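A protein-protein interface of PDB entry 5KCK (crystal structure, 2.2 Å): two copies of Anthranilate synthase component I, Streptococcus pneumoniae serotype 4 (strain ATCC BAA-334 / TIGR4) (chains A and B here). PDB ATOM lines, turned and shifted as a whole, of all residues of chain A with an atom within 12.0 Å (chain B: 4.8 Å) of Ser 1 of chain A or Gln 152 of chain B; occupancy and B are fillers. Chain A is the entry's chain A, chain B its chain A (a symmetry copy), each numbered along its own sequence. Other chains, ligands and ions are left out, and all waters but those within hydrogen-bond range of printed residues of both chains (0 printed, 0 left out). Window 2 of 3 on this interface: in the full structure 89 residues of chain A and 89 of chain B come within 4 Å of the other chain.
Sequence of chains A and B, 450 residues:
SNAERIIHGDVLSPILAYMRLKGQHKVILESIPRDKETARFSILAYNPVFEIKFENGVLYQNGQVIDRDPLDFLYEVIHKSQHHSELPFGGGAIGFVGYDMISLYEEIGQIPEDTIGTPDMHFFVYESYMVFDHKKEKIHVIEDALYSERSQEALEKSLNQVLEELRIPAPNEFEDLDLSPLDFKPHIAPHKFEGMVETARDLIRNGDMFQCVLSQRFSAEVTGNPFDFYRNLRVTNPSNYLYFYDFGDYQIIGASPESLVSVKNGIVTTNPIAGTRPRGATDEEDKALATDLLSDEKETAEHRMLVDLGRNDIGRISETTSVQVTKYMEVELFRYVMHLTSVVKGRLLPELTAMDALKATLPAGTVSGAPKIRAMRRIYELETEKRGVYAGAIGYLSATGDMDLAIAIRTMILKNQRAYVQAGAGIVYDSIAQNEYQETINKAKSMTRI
The backbone NH (N) of Ala 145 of chain B sits at hydrogen-bond distance from the backbone carbonyl oxygen (O) of Ser 1 of chain A (3.5 Å). OD1 of Asp 144 of chain B sits close to O of Ser 1 of chain A, at 2.6 Å. OE2 of Glu 156 of chain B is in salt-bridge range of NH2 of Arg 5 of chain A. The backbone carbonyl oxygen of Asn 2 of chain A sits at hydrogen-bond distance from the side-chain amide nitrogen of Gln 152 of chain B (3.4 Å). N of Ser 1 of chain A sits at hydrogen-bond distance from OE1 of Gln 152 of chain B, 3.3 Å away. OD2 of Asp 144 of chain B sits at hydrogen-bond distance from ND2 of Asn 2 of chain A.
Among the printed residues, pairs that only touch across the chains: Ala 3 of chain A with Glu 156 of chain B (3.5 Å), Asn 2 of chain A with Leu 155 of chain B (3.5 Å), Ala 3 of chain A with Gln 152 of chain B (3.7 Å), Ser 1 of chain A with Leu 155 of chain B (3.8 Å) and Ala 3 of chain A with Leu 155 of chain B (3.9 Å).
Of the 9 printed residues of chain B, 5 touch a printed residue of chain A. Printed residues of chain B that touch a printed residue of chain A: Asp 144, Ala 145, Gln 152, Leu 155 and Glu 156. Hydrophobic or aromatic side chains of chain B within 4 Å of the printed part of chain A: Leu 155. Printed residues of chain A that touch a printed residue of chain B: Ser 1, Asn 2, Ala 3 and Arg 5. Hydrophobic or aromatic side chains of chain A within 4 Å of the printed part of chain B: Ala 3. Among the printed residues, 11 pairs touch across the chains. Among the printed residues, Asp or Glu carboxylates within 4 Å of a Lys or Arg side-chain nitrogen of the other chain: Arg 5 of chain A with Glu 156 of chain B (3.3 Å).
The backbone carbonyl oxygen (O) of Asp 144 of chain B is in hydrogen-bond range of the guanidinium group (NH2) of Arg 150 of chain B, at 2.8 Å.
Ser 1 of chain A touches four residues of chain B. Gln 152 of chain B touches just these residues of chain A: Ser 1, Asn 2 and Ala 3. No residue of chain A comes within 4 Å of Ala 154 of chain B. Of chain A, only Ser 1, Asn 2 and Ala 3 come within 4 Å of Leu 155 of chain B. Of the printed residues of chain A, Glu 156 of chain B touches Ala 3 and Arg 5. Printed residues of chain B within 4 Å of Ala 3 of chain A: Gln 152, Leu 155 and Glu 156. Of the printed residues of chain B, Arg 5 of chain A touches Glu 156 (3.3 Å). Printed residues of chain B within 4 Å of Asn 2 of chain A: Asp 144, Gln 152 and Leu 155. The nearest printed residue of chain B that does not touch Ser 1 of chain A is Arg 150 of chain B (5.3 Å). The nearest residue of chain A that does not touch Gln 152 of chain B is Glu 4 of chain A (6.2 Å). The nearest printed residue of chain B that does not touch Arg 5 of chain A is Leu 155 of chain B (7.2 Å).
No position is printed for both chains. Of the 11 pairs that touch across the chains among the printed residues, none has its exchanged pair printed and touching as well.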
ATOM      1  N   SER A   1      -0.346  18.272  -1.645  1.00  0.00           N
ATOM      2  CA  SER A   1      -0.887  17.013  -1.145  1.00  0.00           C
ATOM      3  C   SER A   1       0.024  15.821  -1.450  1.00  0.00           C
ATOM      4  O   SER A   1      -0.231  14.704  -0.993  1.00  0.00           O
ATOM      5  CB  SER A   1      -2.272  16.760  -1.742  1.00  0.00           C
ATOM      6  OG  SER A   1      -2.186  16.624  -3.154  1.00  0.00           O
ATOM      7  N   ASN A   2       1.071  16.044  -2.244  1.00  0.00           N
ATOM      8  CA  ASN A   2       2.043  14.990  -2.499  1.00  0.00           C
ATOM      9  C   ASN A   2       3.345  15.616  -2.976  1.00  0.00           C
ATOM     10  O   ASN A   2       3.330  16.551  -3.781  1.00  0.00           O
ATOM     11  CB  ASN A   2       1.534  13.979  -3.539  1.00  0.00           C
ATOM     12  CG  ASN A   2       2.561  12.885  -3.849  1.00  0.00           C
ATOM     13  OD1 ASN A   2       3.489  13.091  -4.629  1.00  0.00           O
ATOM     14  ND2 ASN A   2       2.390  11.719  -3.236  1.00  0.00           N
ATOM     15  N   ALA A   3       4.460  15.116  -2.450  1.00  0.00           N
ATOM     16  CA  ALA A   3       5.791  15.464  -2.929  1.00  0.00           C
ATOM     17  C   ALA A   3       6.589  14.172  -3.036  1.00  0.00           C
ATOM     18  O   ALA A   3       6.431  13.276  -2.203  1.00  0.00           O
ATOM     19  CB  ALA A   3       6.499  16.458  -2.000  1.00  0.00           C
ATOM     20  N   GLU A   4       7.435  14.069  -4.058  1.00  0.00           N
ATOM     21  CA  GLU A   4       8.142  12.822  -4.306  1.00  0.00           C
ATOM     22  C   GLU A   4       9.517  13.098  -4.890  1.00  0.00           C
ATOM     23  O   GLU A   4       9.671  13.972  -5.743  1.00  0.00           O
ATOM     24  CB  GLU A   4       7.342  11.922  -5.258  1.00  0.00           C
ATOM     25  CG  GLU A   4       8.083  10.679  -5.725  1.00  0.00           C
ATOM     26  CD  GLU A   4       7.325   9.915  -6.807  1.00  0.00           C
ATOM     27  OE1 GLU A   4       7.118  10.469  -7.913  1.00  0.00           O
ATOM     28  OE2 GLU A   4       6.928   8.763  -6.544  1.00  0.00           O
ATOM     29  N   ARG A   5      10.507  12.337  -4.430  1.00  0.00           N
ATOM     30  CA  ARG A   5      11.817  12.286  -5.059  1.00  0.00           C
ATOM     31  C   ARG A   5      12.097  10.858  -5.507  1.00  0.00           C
ATOM     32  O   ARG A   5      11.814   9.899  -4.780  1.00  0.00           O
ATOM     33  CB  ARG A   5      12.922  12.762  -4.111  1.00  0.00           C
ATOM     34  CG  ARG A   5      14.175  13.251  -4.828  1.00  0.00           C
ATOM     35  CD  ARG A   5      13.936  14.613  -5.478  1.00  0.00           C
ATOM     36  NE  ARG A   5      13.354  15.568  -4.533  1.00  0.00           N
ATOM     37  CZ  ARG A   5      14.037  16.523  -3.902  1.00  0.00           C
ATOM     38  NH1 ARG A   5      15.340  16.669  -4.119  1.00  0.00           N
ATOM     39  NH2 ARG A   5      13.414  17.339  -3.056  1.00  0.00           N
ATOM     40  N   ASP B 144       3.433  12.821   2.058  1.00  0.00           N
ATOM     41  CA  ASP B 144       2.048  13.016   1.644  1.00  0.00           C
ATOM     42  C   ASP B 144       1.269  13.701   2.764  1.00  0.00           C
ATOM     43  O   ASP B 144       1.714  13.744   3.913  1.00  0.00           O
ATOM     44  CB  ASP B 144       1.407  11.670   1.283  1.00  0.00           C
ATOM     45  CG  ASP B 144       0.269  11.808   0.299  1.00  0.00           C
ATOM     46  OD1 ASP B 144      -0.624  12.650   0.537  1.00  0.00           O
ATOM     47  OD2 ASP B 144       0.267  11.070  -0.713  1.00  0.00           O
ATOM     48  N   ALA B 145       0.102  14.262   2.425  1.00  0.00           N
ATOM     49  CA  ALA B 145      -0.712  14.984   3.402  1.00  0.00           C
ATOM     50  C   ALA B 145      -2.049  14.301   3.686  1.00  0.00           C
ATOM     51  O   ALA B 145      -2.984  14.959   4.150  1.00  0.00           O
ATOM     52  CB  ALA B 145      -0.946  16.424   2.949  1.00  0.00           C
ATOM     53  N   ARG B 150      -1.040  18.654   5.811  1.00  0.00           N
ATOM     54  CA  ARG B 150       0.188  19.437   5.718  1.00  0.00           C
ATOM     55  C   ARG B 150       0.207  20.284   4.449  1.00  0.00           C
ATOM     56  O   ARG B 150      -0.273  19.868   3.393  1.00  0.00           O
ATOM     57  CB  ARG B 150       1.408  18.506   5.699  1.00  0.00           C
ATOM     58  CG  ARG B 150       1.853  17.982   7.042  1.00  0.00           C
ATOM     59  CD  ARG B 150       3.199  17.251   6.943  1.00  0.00           C
ATOM     60  NE  ARG B 150       3.154  15.980   6.220  1.00  0.00           N
ATOM     61  CZ  ARG B 150       4.239  15.284   5.870  1.00  0.00           C
ATOM     62  NH1 ARG B 150       5.449  15.740   6.176  1.00  0.00           N
ATOM     63  NH2 ARG B 150       4.117  14.131   5.216  1.00  0.00           N
ATOM     64  N   SER B 151       0.808  21.464   4.546  1.00  0.00           N
ATOM     65  CA  SER B 151       1.028  22.267   3.355  1.00  0.00           C
ATOM     66  C   SER B 151       2.089  21.627   2.460  1.00  0.00           C
ATOM     67  O   SER B 151       2.909  20.814   2.899  1.00  0.00           O
ATOM     68  CB  SER B 151       1.472  23.677   3.724  1.00  0.00           C
ATOM     69  OG  SER B 151       2.867  23.711   3.966  1.00  0.00           O
ATOM     70  N   GLN B 152       2.072  22.027   1.186  1.00  0.00           N
ATOM     71  CA  GLN B 152       3.104  21.593   0.251  1.00  0.00           C
ATOM     72  C   GLN B 152       4.489  22.040   0.708  1.00  0.00           C
ATOM     73  O   GLN B 152       5.480  21.339   0.460  1.00  0.00           O
ATOM     74  CB  GLN B 152       2.795  22.133  -1.146  1.00  0.00           C
ATOM     75  CG  GLN B 152       3.745  21.667  -2.238  1.00  0.00           C
ATOM     76  CD  GLN B 152       3.545  20.211  -2.624  1.00  0.00           C
ATOM     77  OE1 GLN B 152       2.426  19.685  -2.593  1.00  0.00           O
ATOM     78  NE2 GLN B 152       4.638  19.547  -2.992  1.00  0.00           N
ATOM     79  N   GLU B 153       4.574  23.193   1.380  1.00  0.00           N
ATOM     80  CA  GLU B 153       5.844  23.639   1.947  1.00  0.00           C
ATOM     81  C   GLU B 153       6.360  22.654   2.989  1.00  0.00           C
ATOM     82  O   GLU B 153       7.560  22.369   3.044  1.00  0.00           O
ATOM     83  CB  GLU B 153       5.686  25.028   2.571  1.00  0.00           C
ATOM     84  CG  GLU B 153       5.506  26.154   1.574  1.00  0.00           C
ATOM     85  CD  GLU B 153       5.245  27.498   2.245  1.00  0.00           C
ATOM     86  OE1 GLU B 153       4.912  27.517   3.454  1.00  0.00           O
ATOM     87  OE2 GLU B 153       5.373  28.533   1.558  1.00  0.00           O
ATOM     88  N   ALA B 154       5.464  22.126   3.828  1.00  0.00           N
ATOM     89  CA  ALA B 154       5.874  21.171   4.849  1.00  0.00           C
ATOM     90  C   ALA B 154       6.318  19.844   4.234  1.00  0.00           C
ATOM     91  O   ALA B 154       7.250  19.205   4.738  1.00  0.00           O
ATOM     92  CB  ALA B 154       4.735  20.949   5.844  1.00  0.00           C
ATOM     93  N   LEU B 155       5.650  19.397   3.162  1.00  0.00           N
ATOM     94  CA  LEU B 155       6.084  18.170   2.497  1.00  0.00           C
ATOM     95  C   LEU B 155       7.494  18.328   1.952  1.00  0.00           C
ATOM     96  O   LEU B 155       8.337  17.439   2.112  1.00  0.00           O
ATOM     97  CB  LEU B 155       5.126  17.799   1.369  1.00  0.00           C
ATOM     98  CG  LEU B 155       3.638  17.733   1.716  1.00  0.00           C
ATOM     99  CD1 LEU B 155       2.797  17.574   0.452  1.00  0.00           C
ATOM    100  CD2 LEU B 155       3.380  16.584   2.676  1.00  0.00           C
ATOM    101  N   GLU B 156       7.777  19.471   1.329  1.00  0.00           N
ATOM    102  CA  GLU B 156       9.087  19.670   0.728  1.00  0.00           C
ATOM    103  C   GLU B 156      10.183  19.721   1.788  1.00  0.00           C
ATOM    104  O   GLU B 156      11.281  19.191   1.576  1.00  0.00           O
ATOM    105  CB  GLU B 156       9.073  20.937  -0.126  1.00  0.00           C
ATOM    106  CG  GLU B 156       9.938  20.856  -1.382  1.00  0.00           C
ATOM    107  CD  GLU B 156       9.589  19.670  -2.281  1.00  0.00           C
ATOM    108  OE1 GLU B 156       8.385  19.404  -2.509  1.00  0.00           O
ATOM    109  OE2 GLU B 156      10.531  18.999  -2.757  1.00  0.00           O
